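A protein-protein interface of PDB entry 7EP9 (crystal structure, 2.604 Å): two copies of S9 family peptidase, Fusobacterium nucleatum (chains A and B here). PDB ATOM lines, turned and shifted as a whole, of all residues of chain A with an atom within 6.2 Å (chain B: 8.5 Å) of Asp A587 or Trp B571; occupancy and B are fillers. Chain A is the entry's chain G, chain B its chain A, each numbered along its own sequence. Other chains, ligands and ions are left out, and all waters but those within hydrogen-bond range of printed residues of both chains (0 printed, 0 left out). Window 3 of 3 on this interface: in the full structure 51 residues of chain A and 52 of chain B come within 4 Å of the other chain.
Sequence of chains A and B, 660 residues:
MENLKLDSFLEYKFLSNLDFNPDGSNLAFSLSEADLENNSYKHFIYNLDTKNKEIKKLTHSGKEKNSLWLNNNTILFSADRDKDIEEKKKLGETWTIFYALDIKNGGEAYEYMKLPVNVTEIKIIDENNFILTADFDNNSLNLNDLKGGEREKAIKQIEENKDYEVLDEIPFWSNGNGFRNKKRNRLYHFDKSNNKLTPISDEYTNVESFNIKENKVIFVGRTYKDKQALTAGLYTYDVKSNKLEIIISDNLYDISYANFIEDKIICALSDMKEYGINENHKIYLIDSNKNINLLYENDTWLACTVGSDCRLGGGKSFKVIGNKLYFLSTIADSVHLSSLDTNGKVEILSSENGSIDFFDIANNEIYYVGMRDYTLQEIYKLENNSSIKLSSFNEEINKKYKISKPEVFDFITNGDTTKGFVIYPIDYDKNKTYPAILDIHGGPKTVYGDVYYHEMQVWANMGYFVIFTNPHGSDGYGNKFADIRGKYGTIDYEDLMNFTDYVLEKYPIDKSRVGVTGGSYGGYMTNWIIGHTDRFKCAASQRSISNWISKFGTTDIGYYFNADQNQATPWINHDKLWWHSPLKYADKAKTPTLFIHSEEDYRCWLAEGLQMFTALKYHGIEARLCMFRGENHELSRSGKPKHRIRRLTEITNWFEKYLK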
ATOM      1  N   TRP A 578      -0.732  20.262   8.013  1.00  0.00           N
ATOM      2  CA  TRP A 578       0.434  21.122   7.852  1.00  0.00           C
ATOM      3  C   TRP A 578       0.931  21.645   9.193  1.00  0.00           C
ATOM      4  O   TRP A 578       2.125  21.925   9.343  1.00  0.00           O
ATOM      5  CB  TRP A 578       0.104  22.283   6.912  1.00  0.00           C
ATOM      6  CG  TRP A 578       1.236  23.250   6.715  1.00  0.00           C
ATOM      7  CD1 TRP A 578       1.190  24.606   6.866  1.00  0.00           C
ATOM      8  CD2 TRP A 578       2.580  22.937   6.323  1.00  0.00           C
ATOM      9  NE1 TRP A 578       2.419  25.155   6.596  1.00  0.00           N
ATOM     10  CE2 TRP A 578       3.290  24.152   6.260  1.00  0.00           C
ATOM     11  CE3 TRP A 578       3.251  21.746   6.020  1.00  0.00           C
ATOM     12  CZ2 TRP A 578       4.636  24.211   5.907  1.00  0.00           C
ATOM     13  CZ3 TRP A 578       4.587  21.809   5.673  1.00  0.00           C
ATOM     14  CH2 TRP A 578       5.266  23.032   5.619  1.00  0.00           C
ATOM     15  N   PRO A 582       6.909  19.372  11.113  1.00  0.00           N
ATOM     16  CA  PRO A 582       8.009  20.217  11.604  1.00  0.00           C
ATOM     17  C   PRO A 582       8.626  21.105  10.537  1.00  0.00           C
ATOM     18  O   PRO A 582       9.317  22.070  10.889  1.00  0.00           O
ATOM     19  CB  PRO A 582       9.028  19.199  12.134  1.00  0.00           C
ATOM     20  CG  PRO A 582       8.255  17.925  12.313  1.00  0.00           C
ATOM     21  CD  PRO A 582       7.215  17.940  11.240  1.00  0.00           C
ATOM     22  N   LEU A 583       8.407  20.815   9.251  1.00  0.00           N
ATOM     23  CA  LEU A 583       8.951  21.667   8.197  1.00  0.00           C
ATOM     24  C   LEU A 583       8.353  23.066   8.246  1.00  0.00           C
ATOM     25  O   LEU A 583       8.981  24.027   7.786  1.00  0.00           O
ATOM     26  CB  LEU A 583       8.705  21.031   6.828  1.00  0.00           C
ATOM     27  CG  LEU A 583       9.311  21.733   5.612  1.00  0.00           C
ATOM     28  CD1 LEU A 583      10.827  21.791   5.722  1.00  0.00           C
ATOM     29  CD2 LEU A 583       8.889  21.041   4.326  1.00  0.00           C
ATOM     30  N   LYS A 584       7.150  23.201   8.808  1.00  0.00           N
ATOM     31  CA  LYS A 584       6.494  24.502   8.881  1.00  0.00           C
ATOM     32  C   LYS A 584       7.285  25.488   9.731  1.00  0.00           C
ATOM     33  O   LYS A 584       7.187  26.704   9.525  1.00  0.00           O
ATOM     34  CB  LYS A 584       5.079  24.330   9.434  1.00  0.00           C
ATOM     35  CG  LYS A 584       4.234  25.589   9.441  1.00  0.00           C
ATOM     36  CD  LYS A 584       2.891  25.337  10.106  1.00  0.00           C
ATOM     37  CE  LYS A 584       2.156  26.636  10.378  1.00  0.00           C
ATOM     38  NZ  LYS A 584       0.873  26.404  11.095  1.00  0.00           N
ATOM     39  N   TYR A 585       8.080  24.989  10.677  1.00  0.00           N
ATOM     40  CA  TYR A 585       8.810  25.830  11.616  1.00  0.00           C
ATOM     41  C   TYR A 585      10.311  25.836  11.345  1.00  0.00           C
ATOM     42  O   TYR A 585      11.095  26.211  12.223  1.00  0.00           O
ATOM     43  CB  TYR A 585       8.527  25.377  13.049  1.00  0.00           C
ATOM     44  CG  TYR A 585       7.071  25.046  13.292  1.00  0.00           C
ATOM     45  CD1 TYR A 585       6.176  26.024  13.700  1.00  0.00           C
ATOM     46  CD2 TYR A 585       6.591  23.755  13.102  1.00  0.00           C
ATOM     47  CE1 TYR A 585       4.843  25.728  13.919  1.00  0.00           C
ATOM     48  CE2 TYR A 585       5.261  23.451  13.316  1.00  0.00           C
ATOM     49  CZ  TYR A 585       4.392  24.440  13.726  1.00  0.00           C
ATOM     50  OH  TYR A 585       3.067  24.140  13.942  1.00  0.00           O
ATOM     51  N   ALA A 586      10.725  25.434  10.140  1.00  0.00           N
ATOM     52  CA  ALA A 586      12.146  25.400   9.816  1.00  0.00           C
ATOM     53  C   ALA A 586      12.757  26.795   9.792  1.00  0.00           C
ATOM     54  O   ALA A 586      13.961  26.945  10.028  1.00  0.00           O
ATOM     55  CB  ALA A 586      12.359  24.702   8.474  1.00  0.00           C
ATOM     56  N   ASP A 587      11.953  27.823   9.511  1.00  0.00           N
ATOM     57  CA  ASP A 587      12.462  29.189   9.528  1.00  0.00           C
ATOM     58  C   ASP A 587      12.860  29.641  10.927  1.00  0.00           C
ATOM     59  O   ASP A 587      13.622  30.603  11.061  1.00  0.00           O
ATOM     60  CB  ASP A 587      11.424  30.149   8.942  1.00  0.00           C
ATOM     61  CG  ASP A 587      10.094  30.091   9.671  1.00  0.00           C
ATOM     62  OD1 ASP A 587       9.910  29.193  10.520  1.00  0.00           O
ATOM     63  OD2 ASP A 587       9.229  30.948   9.394  1.00  0.00           O
ATOM     64  N   LYS A 588      12.358  28.973  11.964  1.00  0.00           N
ATOM     65  CA  LYS A 588      12.731  29.263  13.341  1.00  0.00           C
ATOM     66  C   LYS A 588      13.816  28.333  13.864  1.00  0.00           C
ATOM     67  O   LYS A 588      14.211  28.454  15.027  1.00  0.00           O
ATOM     68  CB  LYS A 588      11.498  29.179  14.248  1.00  0.00           C
ATOM     69  CG  LYS A 588      10.342  30.055  13.798  1.00  0.00           C
ATOM     70  CD  LYS A 588       9.182  29.993  14.778  1.00  0.00           C
ATOM     71  CE  LYS A 588       8.116  31.019  14.432  1.00  0.00           C
ATOM     72  NZ  LYS A 588       6.800  30.380  14.149  1.00  0.00           N
ATOM     73  N   ALA A 589      14.306  27.414  13.036  1.00  0.00           N
ATOM     74  CA  ALA A 589      15.333  26.474  13.463  1.00  0.00           C
ATOM     75  C   ALA A 589      16.697  27.150  13.468  1.00  0.00           C
ATOM     76  O   ALA A 589      17.129  27.710  12.456  1.00  0.00           O
ATOM     77  CB  ALA A 589      15.351  25.251  12.547  1.00  0.00           C
ATOM     78  N   LYS A 590      17.372  27.101  14.617  1.00  0.00           N
ATOM     79  CA  LYS A 590      18.716  27.638  14.760  1.00  0.00           C
ATOM     80  C   LYS A 590      19.714  26.598  15.244  1.00  0.00           C
ATOM     81  O   LYS A 590      20.909  26.903  15.339  1.00  0.00           O
ATOM     82  CB  LYS A 590      18.715  28.833  15.725  1.00  0.00           C
ATOM     83  CG  LYS A 590      17.612  29.847  15.464  1.00  0.00           C
ATOM     84  CD  LYS A 590      17.783  30.515  14.108  1.00  0.00           C
ATOM     85  CE  LYS A 590      16.708  31.565  13.871  1.00  0.00           C
ATOM     86  NZ  LYS A 590      16.967  32.355  12.635  1.00  0.00           N
ATOM     87  N   GLN A 611      14.114  17.578   2.881  1.00  0.00           N
ATOM     88  CA  GLN A 611      13.420  18.852   3.034  1.00  0.00           C
ATOM     89  C   GLN A 611      13.923  19.617   4.253  1.00  0.00           C
ATOM     90  O   GLN A 611      14.192  20.821   4.173  1.00  0.00           O
ATOM     91  CB  GLN A 611      11.912  18.618   3.126  1.00  0.00           C
ATOM     92  CG  GLN A 611      11.261  18.283   1.796  1.00  0.00           C
ATOM     93  CD  GLN A 611       9.774  18.027   1.921  1.00  0.00           C
ATOM     94  OE1 GLN A 611       8.961  18.942   1.790  1.00  0.00           O
ATOM     95  NE2 GLN A 611       9.408  16.777   2.179  1.00  0.00           N
ATOM     96  N   THR A 614      17.536  20.873   3.413  1.00  0.00           N
ATOM     97  CA  THR A 614      17.515  21.997   2.482  1.00  0.00           C
ATOM     98  C   THR A 614      16.931  23.242   3.138  1.00  0.00           C
ATOM     99  O   THR A 614      17.396  24.362   2.892  1.00  0.00           O
ATOM    100  CB  THR A 614      16.723  21.625   1.227  1.00  0.00           C
ATOM    101  OG1 THR A 614      17.425  20.607   0.502  1.00  0.00           O
ATOM    102  CG2 THR A 614      16.531  22.836   0.323  1.00  0.00           C
ATOM    103  N   ALA A 615      15.922  23.065   3.994  1.00  0.00           N
ATOM    104  CA  ALA A 615      15.326  24.204   4.684  1.00  0.00           C
ATOM    105  C   ALA A 615      16.320  24.858   5.635  1.00  0.00           C
ATOM    106  O   ALA A 615      16.395  26.091   5.710  1.00  0.00           O
ATOM    107  CB  ALA A 615      14.074  23.763   5.439  1.00  0.00           C
ATOM    108  N   TYR A 618      18.876  26.614   3.742  1.00  0.00           N
ATOM    109  CA  TYR A 618      18.280  27.794   3.130  1.00  0.00           C
ATOM    110  C   TYR A 618      18.255  28.976   4.090  1.00  0.00           C
ATOM    111  O   TYR A 618      18.319  30.131   3.651  1.00  0.00           O
ATOM    112  CB  TYR A 618      16.865  27.471   2.649  1.00  0.00           C
ATOM    113  CG  TYR A 618      16.172  28.616   1.953  1.00  0.00           C
ATOM    114  CD1 TYR A 618      16.641  29.106   0.741  1.00  0.00           C
ATOM    115  CD2 TYR A 618      15.047  29.208   2.508  1.00  0.00           C
ATOM    116  CE1 TYR A 618      16.007  30.155   0.104  1.00  0.00           C
ATOM    117  CE2 TYR A 618      14.408  30.255   1.879  1.00  0.00           C
ATOM    118  CZ  TYR A 618      14.891  30.725   0.678  1.00  0.00           C
ATOM    119  OH  TYR A 618      14.251  31.769   0.054  1.00  0.00           O
ATOM    120  N   HIS A 619      18.169  28.713   5.394  1.00  0.00           N
ATOM    121  CA  HIS A 619      18.101  29.761   6.403  1.00  0.00           C
ATOM    122  C   HIS A 619      19.453  30.032   7.058  1.00  0.00           C
ATOM    123  O   HIS A 619      19.505  30.661   8.120  1.00  0.00           O
ATOM    124  CB  HIS A 619      17.055  29.404   7.460  1.00  0.00           C
ATOM    125  CG  HIS A 619      15.645  29.492   6.963  1.00  0.00           C
ATOM    126  ND1 HIS A 619      14.964  28.403   6.464  1.00  0.00           N
ATOM    127  CD2 HIS A 619      14.791  30.538   6.885  1.00  0.00           C
ATOM    128  CE1 HIS A 619      13.749  28.775   6.100  1.00  0.00           C
ATOM    129  NE2 HIS A 619      13.618  30.066   6.346  1.00  0.00           N
ATOM    130  N   ILE B 170      23.388  23.608  -0.289  1.00  0.00           N
ATOM    131  CA  ILE B 170      21.954  23.520  -0.559  1.00  0.00           C
ATOM    132  C   ILE B 170      21.645  23.050  -1.982  1.00  0.00           C
ATOM    133  O   ILE B 170      20.567  22.475  -2.197  1.00  0.00           O
ATOM    134  CB  ILE B 170      21.243  24.843  -0.204  1.00  0.00           C
ATOM    135  CG1 ILE B 170      19.725  24.660  -0.206  1.00  0.00           C
ATOM    136  CG2 ILE B 170      21.643  25.988  -1.108  1.00  0.00           C
ATOM    137  CD1 ILE B 170      18.974  25.909   0.146  1.00  0.00           C
ATOM    138  N   ILE B 549       5.810  22.702  -2.217  1.00  0.00           N
ATOM    139  CA  ILE B 549       6.527  22.666  -0.945  1.00  0.00           C
ATOM    140  C   ILE B 549       7.526  21.517  -0.932  1.00  0.00           C
ATOM    141  O   ILE B 549       8.711  21.705  -0.630  1.00  0.00           O
ATOM    142  CB  ILE B 549       5.537  22.566   0.229  1.00  0.00           C
ATOM    143  CG1 ILE B 549       4.664  23.822   0.307  1.00  0.00           C
ATOM    144  CG2 ILE B 549       6.283  22.346   1.538  1.00  0.00           C
ATOM    145  CD1 ILE B 549       3.301  23.662  -0.333  1.00  0.00           C
ATOM    146  N   PHE B 552      10.353  22.199  -3.134  1.00  0.00           N
ATOM    147  CA  PHE B 552      11.287  23.232  -2.697  1.00  0.00           C
ATOM    148  C   PHE B 552      12.556  22.623  -2.111  1.00  0.00           C
ATOM    149  O   PHE B 552      13.664  23.099  -2.381  1.00  0.00           O
ATOM    150  CB  PHE B 552      10.606  24.149  -1.677  1.00  0.00           C
ATOM    151  CG  PHE B 552      11.498  25.232  -1.126  1.00  0.00           C
ATOM    152  CD1 PHE B 552      12.307  24.996  -0.023  1.00  0.00           C
ATOM    153  CD2 PHE B 552      11.511  26.494  -1.697  1.00  0.00           C
ATOM    154  CE1 PHE B 552      13.122  25.989   0.486  1.00  0.00           C
ATOM    155  CE2 PHE B 552      12.321  27.495  -1.189  1.00  0.00           C
ATOM    156  CZ  PHE B 552      13.130  27.241  -0.097  1.00  0.00           C
ATOM    157  N   GLY B 553      12.416  21.571  -1.311  1.00  0.00           N
ATOM    158  CA  GLY B 553      13.543  21.018  -0.596  1.00  0.00           C
ATOM    159  C   GLY B 553      14.234  19.836  -1.230  1.00  0.00           C
ATOM    160  O   GLY B 553      15.140  19.268  -0.613  1.00  0.00           O
ATOM    161  N   TYR B 559      14.897  25.477  -4.485  1.00  0.00           N
ATOM    162  CA  TYR B 559      14.826  26.407  -3.364  1.00  0.00           C
ATOM    163  C   TYR B 559      14.833  27.869  -3.795  1.00  0.00           C
ATOM    164  O   TYR B 559      14.568  28.739  -2.958  1.00  0.00           O
ATOM    165  CB  TYR B 559      15.966  26.143  -2.378  1.00  0.00           C
ATOM    166  CG  TYR B 559      17.336  26.562  -2.856  1.00  0.00           C
ATOM    167  CD1 TYR B 559      18.119  25.704  -3.614  1.00  0.00           C
ATOM    168  CD2 TYR B 559      17.855  27.810  -2.532  1.00  0.00           C
ATOM    169  CE1 TYR B 559      19.376  26.079  -4.046  1.00  0.00           C
ATOM    170  CE2 TYR B 559      19.110  28.194  -2.959  1.00  0.00           C
ATOM    171  CZ  TYR B 559      19.866  27.325  -3.716  1.00  0.00           C
ATOM    172  OH  TYR B 559      21.118  27.702  -4.146  1.00  0.00           O
ATOM    173  N   ALA B 568       5.955  32.698  -3.719  1.00  0.00           N
ATOM    174  CA  ALA B 568       5.621  32.133  -2.424  1.00  0.00           C
ATOM    175  C   ALA B 568       6.785  31.277  -1.943  1.00  0.00           C
ATOM    176  O   ALA B 568       7.781  31.088  -2.646  1.00  0.00           O
ATOM    177  CB  ALA B 568       4.322  31.327  -2.492  1.00  0.00           C
ATOM    178  N   THR B 569       6.637  30.744  -0.730  1.00  0.00           N
ATOM    179  CA  THR B 569       7.702  30.049  -0.027  1.00  0.00           C
ATOM    180  C   THR B 569       7.036  29.250   1.078  1.00  0.00           C
ATOM    181  O   THR B 569       6.043  29.729   1.644  1.00  0.00           O
ATOM    182  CB  THR B 569       8.718  31.057   0.537  1.00  0.00           C
ATOM    183  OG1 THR B 569       9.614  31.467  -0.504  1.00  0.00           O
ATOM    184  CG2 THR B 569       9.519  30.482   1.688  1.00  0.00           C
ATOM    185  N   PRO B 570       7.518  28.033   1.402  1.00  0.00           N
ATOM    186  CA  PRO B 570       6.862  27.231   2.447  1.00  0.00           C
ATOM    187  C   PRO B 570       6.699  27.954   3.778  1.00  0.00           C
ATOM    188  O   PRO B 570       6.011  27.460   4.676  1.00  0.00           O
ATOM    189  CB  PRO B 570       7.793  26.019   2.588  1.00  0.00           C
ATOM    190  CG  PRO B 570       8.427  25.886   1.253  1.00  0.00           C
ATOM    191  CD  PRO B 570       8.609  27.289   0.744  1.00  0.00           C
ATOM    192  N   TRP B 571       7.320  29.127   3.916  1.00  0.00           N
ATOM    193  CA  TRP B 571       7.228  29.913   5.135  1.00  0.00           C
ATOM    194  C   TRP B 571       6.756  31.345   4.916  1.00  0.00           C
ATOM    195  O   TRP B 571       6.494  32.040   5.904  1.00  0.00           O
ATOM    196  CB  TRP B 571       8.584  29.925   5.858  1.00  0.00           C
ATOM    197  CG  TRP B 571       9.143  28.543   6.036  1.00  0.00           C
ATOM    198  CD1 TRP B 571       8.883  27.681   7.062  1.00  0.00           C
ATOM    199  CD2 TRP B 571      10.036  27.853   5.151  1.00  0.00           C
ATOM    200  NE1 TRP B 571       9.565  26.504   6.876  1.00  0.00           N
ATOM    201  CE2 TRP B 571      10.280  26.584   5.710  1.00  0.00           C
ATOM    202  CE3 TRP B 571      10.657  28.190   3.945  1.00  0.00           C
ATOM    203  CZ2 TRP B 571      11.118  25.650   5.103  1.00  0.00           C
ATOM    204  CZ3 TRP B 571      11.488  27.261   3.343  1.00  0.00           C
ATOM    205  CH2 TRP B 571      11.710  26.007   3.923  1.00  0.00           C
ATOM    206  N   ILE B 572       6.636  31.806   3.673  1.00  0.00           N
ATOM    207  CA  ILE B 572       6.081  33.119   3.354  1.00  0.00           C
ATOM    208  C   ILE B 572       4.956  32.903   2.353  1.00  0.00           C
ATOM    209  O   ILE B 572       5.205  32.481   1.217  1.00  0.00           O
ATOM    210  CB  ILE B 572       7.135  34.084   2.793  1.00  0.00           C
ATOM    211  CG1 ILE B 572       8.345  34.164   3.724  1.00  0.00           C
ATOM    212  CG2 ILE B 572       6.532  35.467   2.588  1.00  0.00           C
ATOM    213  CD1 ILE B 572       9.432  35.095   3.232  1.00  0.00           C
ATOM    214  N   ASN B 573       3.726  33.201   2.767  1.00  0.00           N
ATOM    215  CA  ASN B 573       2.522  32.933   1.981  1.00  0.00           C
ATOM    216  C   ASN B 573       2.482  31.472   1.533  1.00  0.00           C
ATOM    217  O   ASN B 573       2.477  31.148   0.344  1.00  0.00           O
ATOM    218  CB  ASN B 573       2.412  33.883   0.785  1.00  0.00           C
ATOM    219  CG  ASN B 573       0.971  34.126   0.369  1.00  0.00           C
ATOM    220  OD1 ASN B 573       0.038  33.627   0.999  1.00  0.00           O
ATOM    221  ND2 ASN B 573       0.785  34.897  -0.697  1.00  0.00           N
ATOM    222  N   HIS B 574       2.458  30.584   2.529  1.00  0.00           N
ATOM    223  CA  HIS B 574       2.379  29.154   2.248  1.00  0.00           C
ATOM    224  C   HIS B 574       1.072  28.802   1.547  1.00  0.00           C
ATOM    225  O   HIS B 574       1.042  27.917   0.684  1.00  0.00           O
ATOM    226  CB  HIS B 574       2.525  28.359   3.547  1.00  0.00           C
ATOM    227  CG  HIS B 574       2.091  26.931   3.436  1.00  0.00           C
ATOM    228  ND1 HIS B 574       2.957  25.913   3.099  1.00  0.00           N
ATOM    229  CD2 HIS B 574       0.882  26.350   3.620  1.00  0.00           C
ATOM    230  CE1 HIS B 574       2.300  24.767   3.078  1.00  0.00           C
ATOM    231  NE2 HIS B 574       1.039  25.005   3.390  1.00  0.00           N
ATOM    232  N   ASP B 575      -0.018  29.488   1.903  1.00  0.00           N
ATOM    233  CA  ASP B 575      -1.306  29.209   1.275  1.00  0.00           C
ATOM    234  C   ASP B 575      -1.263  29.457  -0.226  1.00  0.00           C
ATOM    235  O   ASP B 575      -1.980  28.796  -0.983  1.00  0.00           O
ATOM    236  CB  ASP B 575      -2.404  30.056   1.919  1.00  0.00           C
ATOM    237  CG  ASP B 575      -2.605  29.733   3.387  1.00  0.00           C
ATOM    238  OD1 ASP B 575      -2.960  28.579   3.704  1.00  0.00           O
ATOM    239  OD2 ASP B 575      -2.406  30.639   4.224  1.00  0.00           O
ATOM    240  N   LEU B 577       1.631  29.107  -2.165  1.00  0.00           N
ATOM    241  CA  LEU B 577       2.420  28.005  -2.705  1.00  0.00           C
ATOM    242  C   LEU B 577       1.630  26.704  -2.720  1.00  0.00           C
ATOM    243  O   LEU B 577       1.827  25.867  -3.608  1.00  0.00           O
ATOM    244  CB  LEU B 577       3.705  27.833  -1.896  1.00  0.00           C
ATOM    245  CG  LEU B 577       4.859  27.132  -2.612  1.00  0.00           C
ATOM    246  CD1 LEU B 577       5.347  27.961  -3.788  1.00  0.00           C
ATOM    247  CD2 LEU B 577       5.996  26.845  -1.649  1.00  0.00           C
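The backbone carbonyl oxygen (O) of Leu A583 sits at hydrogen-bond distance from the indole nitrogen (NE1) of Trp B571, 2.7 Å away. A ring nitrogen (NE2) of His B574 lies within hydrogen-bond range of the indole nitrogen (NE1) of Trp A578. OG1 of Thr A614 is in hydrogen-bond range of O of Gly B553.
No position is printed for both chains.
O of Ala A615 is in hydrogen-bond range of ND1 of His A619, at 2.8 Å. The backbone carbonyl oxygen (O) of Phe B552 lies within hydrogen-bond range of the backbone NH (N) of Tyr B559 (3.4 Å).
Asp A587 touches one residue of chain B. Of chain A, only Leu A583 (2.7 Å), Lys A584 (3.1 Å), Ala A586 (3.6 Å), Asp A587 (3.7 Å), Ala A615 (3.5 Å) and His A619 (3.8 Å) come within 4 Å of Trp B571. Ala A586 touches just one residue of chain B: Trp B571. Of the printed residues of chain A, Pro B570 touches Trp A578 (3.7 Å). Of the printed residues of chain B, Tyr A618 touches Ile B170, Phe B552 and Tyr B559. The nearest residue of chain B that does not touch Asp A587 is Ile B572 (6.3 Å). The nearest printed residue of chain A that does not touch Gly B553 is Gln A611 (4.01 Å).
Among the printed residues, pairs that only touch across the chains: Trp A578 with Pro B570 (3.7 Å), Lys A584 with Trp B571 (3.1 Å), Ala A586 with Trp B571 (3.6 Å), Asp A587 with Trp B571 (3.7 Å), Gln A611 with Ile B549 (3.7 Å), Thr A614 with Ile B170 (3.5 Å), Thr A614 with Phe B552 (3.9 Å), Ala A615 with Trp B571 (3.5 Å), Tyr A618 with Ile B170 (3.6 Å), Tyr A618 with Phe B552 (3.8 Å), Tyr A618 with Tyr B559 (3.7 Å) and His A619 with Trp B571 (3.8 Å).
Of the 15 printed residues of chain A, 10 touch a printed residue of chain B. Printed residues of chain A that touch a printed residue of chain B: Trp A578, Leu A583, Lys A584, Ala A586, Asp A587, Gln A611, Thr A614, Ala A615, Tyr A618 and His A619. Hydrophobic or aromatic side chains of chain A within 4 Å of the printed part of chain B: Trp A578, Leu A583, Ala A586, Ala A615, Tyr A618 and His A619. Printed residues of chain B that touch a printed residue of chain A: Ile B170, Ile B549, Phe B552, Gly B553, Tyr B559, Pro B570, Trp B571 and His B574. Hydrophobic or aromatic side chains of chain B that line the printed part of chain A: Ile B170, Phe B552, Tyr B559, Trp B571 and His B574. Among the printed residues, 15 pairs touch across the chains. Among the printed residues, no Asp or Glu carboxylate lies within 4 Å of a Lys or Arg side-chain nitrogen of the other chain.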
